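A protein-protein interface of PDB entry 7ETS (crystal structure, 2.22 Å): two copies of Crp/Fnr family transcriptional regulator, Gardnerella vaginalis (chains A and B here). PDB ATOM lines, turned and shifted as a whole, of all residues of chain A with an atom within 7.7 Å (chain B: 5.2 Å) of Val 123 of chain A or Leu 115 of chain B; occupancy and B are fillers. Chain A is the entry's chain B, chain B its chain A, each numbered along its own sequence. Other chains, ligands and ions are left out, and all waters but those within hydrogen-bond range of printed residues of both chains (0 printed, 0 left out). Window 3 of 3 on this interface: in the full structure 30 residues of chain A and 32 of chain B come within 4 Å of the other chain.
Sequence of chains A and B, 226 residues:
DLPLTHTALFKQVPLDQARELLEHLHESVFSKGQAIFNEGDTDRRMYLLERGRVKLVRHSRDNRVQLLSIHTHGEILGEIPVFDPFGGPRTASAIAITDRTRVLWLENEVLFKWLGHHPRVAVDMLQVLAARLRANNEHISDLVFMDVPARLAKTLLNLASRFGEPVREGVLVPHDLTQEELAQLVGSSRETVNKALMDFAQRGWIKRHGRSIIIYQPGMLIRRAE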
ATOM      1  N   GLN A  12      10.930 -24.378  18.161  1.00  0.00           N
ATOM      2  CA  GLN A  12      11.654 -23.218  18.659  1.00  0.00           C
ATOM      3  C   GLN A  12      12.856 -23.609  19.513  1.00  0.00           C
ATOM      4  O   GLN A  12      13.510 -22.736  20.093  1.00  0.00           O
ATOM      5  CB  GLN A  12      10.683 -22.316  19.438  1.00  0.00           C
ATOM      6  CG  GLN A  12      11.204 -20.944  19.870  1.00  0.00           C
ATOM      7  CD  GLN A  12      11.666 -20.081  18.711  1.00  0.00           C
ATOM      8  OE1 GLN A  12      12.812 -19.634  18.675  1.00  0.00           O
ATOM      9  NE2 GLN A  12      10.767 -19.824  17.766  1.00  0.00           N
ATOM     10  N   LEU A 115      14.187 -28.143  31.120  1.00  0.00           N
ATOM     11  CA  LEU A 115      13.448 -26.884  31.090  1.00  0.00           C
ATOM     12  C   LEU A 115      14.048 -25.880  32.062  1.00  0.00           C
ATOM     13  O   LEU A 115      14.041 -24.673  31.802  1.00  0.00           O
ATOM     14  CB  LEU A 115      11.972 -27.120  31.415  1.00  0.00           C
ATOM     15  CG  LEU A 115      11.128 -27.931  30.430  1.00  0.00           C
ATOM     16  CD1 LEU A 115       9.672 -27.944  30.867  1.00  0.00           C
ATOM     17  CD2 LEU A 115      11.265 -27.388  29.019  1.00  0.00           C
ATOM     18  N   HIS A 118      17.083 -24.461  30.345  1.00  0.00           N
ATOM     19  CA  HIS A 118      16.720 -23.626  29.202  1.00  0.00           C
ATOM     20  C   HIS A 118      15.276 -23.170  29.354  1.00  0.00           C
ATOM     21  O   HIS A 118      14.395 -23.593  28.598  1.00  0.00           O
ATOM     22  CB  HIS A 118      16.921 -24.388  27.891  1.00  0.00           C
ATOM     23  CG  HIS A 118      18.193 -25.176  27.840  1.00  0.00           C
ATOM     24  ND1 HIS A 118      19.426 -24.591  27.648  1.00  0.00           N
ATOM     25  CD2 HIS A 118      18.426 -26.505  27.964  1.00  0.00           C
ATOM     26  CE1 HIS A 118      20.362 -25.523  27.654  1.00  0.00           C
ATOM     27  NE2 HIS A 118      19.781 -26.694  27.843  1.00  0.00           N
ATOM     28  N   PRO A 119      14.998 -22.292  30.323  1.00  0.00           N
ATOM     29  CA  PRO A 119      13.603 -21.878  30.561  1.00  0.00           C
ATOM     30  C   PRO A 119      12.976 -21.146  29.395  1.00  0.00           C
ATOM     31  O   PRO A 119      11.745 -21.009  29.361  1.00  0.00           O
ATOM     32  CB  PRO A 119      13.708 -20.969  31.795  1.00  0.00           C
ATOM     33  CG  PRO A 119      15.039 -21.280  32.402  1.00  0.00           C
ATOM     34  CD  PRO A 119      15.929 -21.637  31.255  1.00  0.00           C
ATOM     35  N   ARG A 120      13.775 -20.674  28.437  1.00  0.00           N
ATOM     36  CA  ARG A 120      13.217 -19.926  27.318  1.00  0.00           C
ATOM     37  C   ARG A 120      12.384 -20.812  26.397  1.00  0.00           C
ATOM     38  O   ARG A 120      11.462 -20.322  25.737  1.00  0.00           O
ATOM     39  CB  ARG A 120      14.344 -19.243  26.546  1.00  0.00           C
ATOM     40  CG  ARG A 120      13.900 -18.477  25.310  1.00  0.00           C
ATOM     41  CD  ARG A 120      14.277 -19.231  24.047  1.00  0.00           C
ATOM     42  NE  ARG A 120      13.835 -18.544  22.839  1.00  0.00           N
ATOM     43  CZ  ARG A 120      14.131 -18.940  21.605  1.00  0.00           C
ATOM     44  NH1 ARG A 120      13.685 -18.253  20.564  1.00  0.00           N
ATOM     45  NH2 ARG A 120      14.875 -20.022  21.413  1.00  0.00           N
ATOM     46  N   VAL A 121      12.670 -22.114  26.357  1.00  0.00           N
ATOM     47  CA  VAL A 121      11.886 -22.997  25.498  1.00  0.00           C
ATOM     48  C   VAL A 121      10.476 -23.177  26.049  1.00  0.00           C
ATOM     49  O   VAL A 121       9.518 -23.339  25.283  1.00  0.00           O
ATOM     50  CB  VAL A 121      12.605 -24.349  25.308  1.00  0.00           C
ATOM     51  CG1 VAL A 121      12.680 -25.123  26.607  1.00  0.00           C
ATOM     52  CG2 VAL A 121      11.892 -25.171  24.261  1.00  0.00           C
ATOM     53  N   ALA A 122      10.318 -23.155  27.375  1.00  0.00           N
ATOM     54  CA  ALA A 122       8.988 -23.303  27.957  1.00  0.00           C
ATOM     55  C   ALA A 122       8.089 -22.124  27.614  1.00  0.00           C
ATOM     56  O   ALA A 122       6.864 -22.274  27.570  1.00  0.00           O
ATOM     57  CB  ALA A 122       9.090 -23.474  29.473  1.00  0.00           C
ATOM     58  N   VAL A 123       8.678 -20.951  27.371  1.00  0.00           N
ATOM     59  CA  VAL A 123       7.897 -19.794  26.946  1.00  0.00           C
ATOM     60  C   VAL A 123       7.166 -20.092  25.643  1.00  0.00           C
ATOM     61  O   VAL A 123       5.997 -19.726  25.471  1.00  0.00           O
ATOM     62  CB  VAL A 123       8.802 -18.555  26.811  1.00  0.00           C
ATOM     63  CG1 VAL A 123       8.022 -17.384  26.226  1.00  0.00           C
ATOM     64  CG2 VAL A 123       9.410 -18.178  28.154  1.00  0.00           C
ATOM     65  N   ASP A 124       7.836 -20.758  24.707  1.00  0.00           N
ATOM     66  CA  ASP A 124       7.238 -21.009  23.403  1.00  0.00           C
ATOM     67  C   ASP A 124       6.554 -22.364  23.327  1.00  0.00           C
ATOM     68  O   ASP A 124       5.701 -22.568  22.454  1.00  0.00           O
ATOM     69  CB  ASP A 124       8.303 -20.865  22.320  1.00  0.00           C
ATOM     70  CG  ASP A 124       9.205 -19.663  22.567  1.00  0.00           C
ATOM     71  OD1 ASP A 124      10.437 -19.847  22.661  1.00  0.00           O
ATOM     72  OD2 ASP A 124       8.682 -18.542  22.713  1.00  0.00           O
ATOM     73  N   MET A 125       6.901 -23.290  24.224  1.00  0.00           N
ATOM     74  CA  MET A 125       6.039 -24.439  24.464  1.00  0.00           C
ATOM     75  C   MET A 125       4.755 -24.026  25.165  1.00  0.00           C
ATOM     76  O   MET A 125       3.771 -24.774  25.137  1.00  0.00           O
ATOM     77  CB  MET A 125       6.779 -25.493  25.283  1.00  0.00           C
ATOM     78  CG  MET A 125       7.672 -26.406  24.458  1.00  0.00           C
ATOM     79  SD  MET A 125       8.855 -27.332  25.458  1.00  0.00           S
ATOM     80  CE  MET A 125       7.765 -28.142  26.623  1.00  0.00           C
ATOM     81  N   LEU A 126       4.752 -22.849  25.793  1.00  0.00           N
ATOM     82  CA  LEU A 126       3.534 -22.323  26.393  1.00  0.00           C
ATOM     83  C   LEU A 126       2.568 -21.820  25.327  1.00  0.00           C
ATOM     84  O   LEU A 126       1.350 -21.990  25.455  1.00  0.00           O
ATOM     85  CB  LEU A 126       3.888 -21.206  27.372  1.00  0.00           C
ATOM     86  CG  LEU A 126       2.793 -20.619  28.267  1.00  0.00           C
ATOM     87  CD1 LEU A 126       2.451 -21.584  29.385  1.00  0.00           C
ATOM     88  CD2 LEU A 126       3.223 -19.273  28.829  1.00  0.00           C
ATOM     89  N   GLN A 127       3.092 -21.210  24.263  1.00  0.00           N
ATOM     90  CA  GLN A 127       2.239 -20.618  23.242  1.00  0.00           C
ATOM     91  C   GLN A 127       1.611 -21.664  22.330  1.00  0.00           C
ATOM     92  O   GLN A 127       0.558 -21.397  21.739  1.00  0.00           O
ATOM     93  CB  GLN A 127       3.026 -19.601  22.411  1.00  0.00           C
ATOM     94  CG  GLN A 127       2.199 -18.813  21.405  1.00  0.00           C
ATOM     95  CD  GLN A 127       2.995 -17.709  20.735  1.00  0.00           C
ATOM     96  OE1 GLN A 127       4.150 -17.460  21.081  1.00  0.00           O
ATOM     97  NE2 GLN A 127       2.375 -17.034  19.773  1.00  0.00           N
ATOM     98  N   VAL A 128       2.226 -22.841  22.194  1.00  0.00           N
ATOM     99  CA  VAL A 128       1.600 -23.894  21.404  1.00  0.00           C
ATOM    100  C   VAL A 128       0.501 -24.572  22.209  1.00  0.00           C
ATOM    101  O   VAL A 128      -0.577 -24.860  21.679  1.00  0.00           O
ATOM    102  CB  VAL A 128       2.651 -24.902  20.900  1.00  0.00           C
ATOM    103  CG1 VAL A 128       1.990 -26.054  20.190  1.00  0.00           C
ATOM    104  CG2 VAL A 128       3.656 -24.220  19.974  1.00  0.00           C
ATOM    105  N   LEU A 129       0.741 -24.811  23.502  1.00  0.00           N
ATOM    106  CA  LEU A 129      -0.318 -25.328  24.364  1.00  0.00           C
ATOM    107  C   LEU A 129      -1.493 -24.363  24.419  1.00  0.00           C
ATOM    108  O   LEU A 129      -2.652 -24.788  24.488  1.00  0.00           O
ATOM    109  CB  LEU A 129       0.223 -25.590  25.769  1.00  0.00           C
ATOM    110  CG  LEU A 129       0.516 -27.043  26.143  1.00  0.00           C
ATOM    111  CD1 LEU A 129       1.609 -27.618  25.258  1.00  0.00           C
ATOM    112  CD2 LEU A 129       0.896 -27.159  27.615  1.00  0.00           C
ATOM    113  N   VAL B 110       3.377  -7.078  26.119  1.00  0.00           N
ATOM    114  CA  VAL B 110       3.883  -6.873  27.472  1.00  0.00           C
ATOM    115  C   VAL B 110       4.057  -8.211  28.176  1.00  0.00           C
ATOM    116  O   VAL B 110       5.073  -8.460  28.837  1.00  0.00           O
ATOM    117  CB  VAL B 110       2.947  -5.937  28.259  1.00  0.00           C
ATOM    118  CG1 VAL B 110       3.399  -5.826  29.708  1.00  0.00           C
ATOM    119  CG2 VAL B 110       2.897  -4.566  27.604  1.00  0.00           C
ATOM    120  N   LEU B 111       3.070  -9.100  28.034  1.00  0.00           N
ATOM    121  CA  LEU B 111       3.137 -10.394  28.701  1.00  0.00           C
ATOM    122  C   LEU B 111       4.320 -11.214  28.207  1.00  0.00           C
ATOM    123  O   LEU B 111       5.013 -11.859  29.003  1.00  0.00           O
ATOM    124  CB  LEU B 111       1.833 -11.159  28.485  1.00  0.00           C
ATOM    125  CG  LEU B 111       1.691 -12.480  29.240  1.00  0.00           C
ATOM    126  CD1 LEU B 111       1.612 -12.234  30.741  1.00  0.00           C
ATOM    127  CD2 LEU B 111       0.471 -13.248  28.753  1.00  0.00           C
ATOM    128  N   PHE B 112       4.570 -11.202  26.895  1.00  0.00           N
ATOM    129  CA  PHE B 112       5.647 -12.018  26.342  1.00  0.00           C
ATOM    130  C   PHE B 112       7.010 -11.423  26.665  1.00  0.00           C
ATOM    131  O   PHE B 112       7.974 -12.160  26.906  1.00  0.00           O
ATOM    132  CB  PHE B 112       5.464 -12.176  24.833  1.00  0.00           C
ATOM    133  CG  PHE B 112       4.185 -12.866  24.448  1.00  0.00           C
ATOM    134  CD1 PHE B 112       3.534 -13.702  25.342  1.00  0.00           C
ATOM    135  CD2 PHE B 112       3.632 -12.678  23.192  1.00  0.00           C
ATOM    136  CE1 PHE B 112       2.359 -14.334  24.991  1.00  0.00           C
ATOM    137  CE2 PHE B 112       2.458 -13.307  22.835  1.00  0.00           C
ATOM    138  CZ  PHE B 112       1.821 -14.136  23.736  1.00  0.00           C
ATOM    139  N   LYS B 113       7.114 -10.090  26.658  1.00  0.00           N
ATOM    140  CA  LYS B 113       8.321  -9.442  27.159  1.00  0.00           C
ATOM    141  C   LYS B 113       8.555  -9.790  28.621  1.00  0.00           C
ATOM    142  O   LYS B 113       9.678 -10.124  29.018  1.00  0.00           O
ATOM    143  CB  LYS B 113       8.213  -7.927  26.981  1.00  0.00           C
ATOM    144  CG  LYS B 113       9.219  -7.133  27.802  1.00  0.00           C
ATOM    145  CD  LYS B 113       8.774  -5.687  27.967  1.00  0.00           C
ATOM    146  CE  LYS B 113       7.381  -5.603  28.586  1.00  0.00           C
ATOM    147  NZ  LYS B 113       7.298  -6.234  29.934  1.00  0.00           N
ATOM    148  N   TRP B 114       7.497  -9.726  29.436  1.00  0.00           N
ATOM    149  CA  TRP B 114       7.619 -10.051  30.852  1.00  0.00           C
ATOM    150  C   TRP B 114       8.014 -11.508  31.049  1.00  0.00           C
ATOM    151  O   TRP B 114       8.878 -11.816  31.880  1.00  0.00           O
ATOM    152  CB  TRP B 114       6.304  -9.739  31.566  1.00  0.00           C
ATOM    153  CG  TRP B 114       6.318 -10.008  33.037  1.00  0.00           C
ATOM    154  CD1 TRP B 114       6.845  -9.211  34.014  1.00  0.00           C
ATOM    155  CD2 TRP B 114       5.765 -11.148  33.704  1.00  0.00           C
ATOM    156  NE1 TRP B 114       6.660  -9.790  35.246  1.00  0.00           N
ATOM    157  CE2 TRP B 114       6.000 -10.980  35.085  1.00  0.00           C
ATOM    158  CE3 TRP B 114       5.098 -12.297  33.268  1.00  0.00           C
ATOM    159  CZ2 TRP B 114       5.591 -11.917  36.031  1.00  0.00           C
ATOM    160  CZ3 TRP B 114       4.692 -13.226  34.208  1.00  0.00           C
ATOM    161  CH2 TRP B 114       4.940 -13.032  35.574  1.00  0.00           C
ATOM    162  N   LEU B 115       7.394 -12.419  30.292  1.00  0.00           N
ATOM    163  CA  LEU B 115       7.776 -13.823  30.369  1.00  0.00           C
ATOM    164  C   LEU B 115       9.194 -14.043  29.866  1.00  0.00           C
ATOM    165  O   LEU B 115       9.891 -14.938  30.356  1.00  0.00           O
ATOM    166  CB  LEU B 115       6.788 -14.684  29.582  1.00  0.00           C
ATOM    167  CG  LEU B 115       5.413 -14.878  30.227  1.00  0.00           C
ATOM    168  CD1 LEU B 115       4.468 -15.565  29.260  1.00  0.00           C
ATOM    169  CD2 LEU B 115       5.539 -15.672  31.518  1.00  0.00           C
ATOM    170  N   GLY B 116       9.638 -13.245  28.892  1.00  0.00           N
ATOM    171  CA  GLY B 116      11.026 -13.315  28.478  1.00  0.00           C
ATOM    172  C   GLY B 116      11.980 -12.855  29.560  1.00  0.00           C
ATOM    173  O   GLY B 116      13.100 -13.364  29.662  1.00  0.00           O
ATOM    174  N   HIS B 117      11.551 -11.899  30.388  1.00  0.00           N
ATOM    175  CA  HIS B 117      12.391 -11.439  31.487  1.00  0.00           C
ATOM    176  C   HIS B 117      12.461 -12.477  32.599  1.00  0.00           C
ATOM    177  O   HIS B 117      13.509 -12.647  33.230  1.00  0.00           O
ATOM    178  CB  HIS B 117      11.868 -10.106  32.028  1.00  0.00           C
ATOM    179  CG  HIS B 117      12.069  -8.954  31.094  1.00  0.00           C
ATOM    180  ND1 HIS B 117      11.422  -7.747  31.251  1.00  0.00           N
ATOM    181  CD2 HIS B 117      12.849  -8.823  29.996  1.00  0.00           C
ATOM    182  CE1 HIS B 117      11.791  -6.924  30.286  1.00  0.00           C
ATOM    183  NE2 HIS B 117      12.657  -7.551  29.511  1.00  0.00           N
ATOM    184  N   HIS B 118      11.358 -13.180  32.853  1.00  0.00           N
ATOM    185  CA  HIS B 118      11.291 -14.227  33.871  1.00  0.00           C
ATOM    186  C   HIS B 118      10.842 -15.527  33.210  1.00  0.00           C
ATOM    187  O   HIS B 118       9.695 -15.964  33.388  1.00  0.00           O
ATOM    188  CB  HIS B 118      10.340 -13.841  35.003  1.00  0.00           C
ATOM    189  CG  HIS B 118      10.373 -12.386  35.353  1.00  0.00           C
ATOM    190  ND1 HIS B 118      11.415 -11.810  36.045  1.00  0.00           N
ATOM    191  CD2 HIS B 118       9.488 -11.392  35.107  1.00  0.00           C
ATOM    192  CE1 HIS B 118      11.173 -10.521  36.208  1.00  0.00           C
ATOM    193  NE2 HIS B 118      10.010 -10.243  35.649  1.00  0.00           N
ATOM    194  N   PRO B 119      11.724 -16.175  32.440  1.00  0.00           N
ATOM    195  CA  PRO B 119      11.313 -17.395  31.726  1.00  0.00           C
ATOM    196  C   PRO B 119      11.034 -18.575  32.639  1.00  0.00           C
ATOM    197  O   PRO B 119      10.414 -19.546  32.188  1.00  0.00           O
ATOM    198  CB  PRO B 119      12.501 -17.675  30.796  1.00  0.00           C
ATOM    199  CG  PRO B 119      13.666 -17.042  31.479  1.00  0.00           C
ATOM    200  CD  PRO B 119      13.130 -15.821  32.173  1.00  0.00           C
ATOM    201  N   VAL B 121       8.982 -18.452  35.027  1.00  0.00           N
ATOM    202  CA  VAL B 121       7.545 -18.380  35.273  1.00  0.00           C
ATOM    203  C   VAL B 121       6.780 -19.198  34.237  1.00  0.00           C
ATOM    204  O   VAL B 121       5.788 -19.862  34.561  1.00  0.00           O
ATOM    205  CB  VAL B 121       7.087 -16.910  35.286  1.00  0.00           C
ATOM    206  CG1 VAL B 121       5.587 -16.815  35.492  1.00  0.00           C
ATOM    207  CG2 VAL B 121       7.827 -16.134  36.366  1.00  0.00           C
ATOM    208  N   ALA B 122       7.228 -19.165  32.980  1.00  0.00           N
ATOM    209  CA  ALA B 122       6.544 -19.917  31.931  1.00  0.00           C
ATOM    210  C   ALA B 122       6.627 -21.420  32.168  1.00  0.00           C
ATOM    211  O   ALA B 122       5.759 -22.168  31.705  1.00  0.00           O
ATOM    212  CB  ALA B 122       7.127 -19.565  30.563  1.00  0.00           C
ATOM    213  N   MET B 125       3.684 -21.888  34.486  1.00  0.00           N
ATOM    214  CA  MET B 125       2.458 -21.711  33.716  1.00  0.00           C
ATOM    215  C   MET B 125       2.253 -22.853  32.734  1.00  0.00           C
ATOM    216  O   MET B 125       1.113 -23.159  32.368  1.00  0.00           O
ATOM    217  CB  MET B 125       2.486 -20.380  32.968  1.00  0.00           C
ATOM    218  CG  MET B 125       2.405 -19.163  33.862  1.00  0.00           C
ATOM    219  SD  MET B 125       2.260 -17.639  32.910  1.00  0.00           S
ATOM    220  CE  MET B 125       2.198 -16.431  34.228  1.00  0.00           C
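Of the 13 printed residues of chain B, 4 touch a printed residue of chain A. Hydrophobic or aromatic side chains of chain B within 4 Å of the printed part of chain A: Leu 115, Pro 119, Ala 122 and Met 125. Among the printed residues, 5 pairs touch across the chains. Among the printed residues, no Asp or Glu carboxylate lies within 4 Å of a Lys or Arg side-chain nitrogen of the other chain.
Printed residues of chain B within 4 Å of Pro 119 of chain A: Pro 119. Of chain B, only Leu 115 and Ala 122 come within 4 Å of Val 123 of chain A. Leu 115 of chain B touches just these residues of chain A: Val 123 and Leu 126. His 118 of chain B touches none of the printed residues of chain A. Printed residues of chain A within 4 Å of Pro 119 of chain B: Pro 119 (3.5 Å).
Val 123 of chain A touches Leu 115 of chain B. Val 123 of chain A touches Ala 122 of chain B (CG2 to CB, 3.6 Å). Leu 126 of chain A touches Leu 115 of chain B (CD2 to CD1, 3.9 Å). Met 125 of chain B touches Leu 126 of chain A.
Pro 119 of chain B touches its own counterpart, Pro 119 of chain A. Positions printed for both chains: 115, 118, 119, 121, 122 and 125.
The backbone carbonyl oxygen of Pro 119 of chain A sits close to the backbone carbonyl oxygen of Pro 119 of chain B (3.5 Å).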
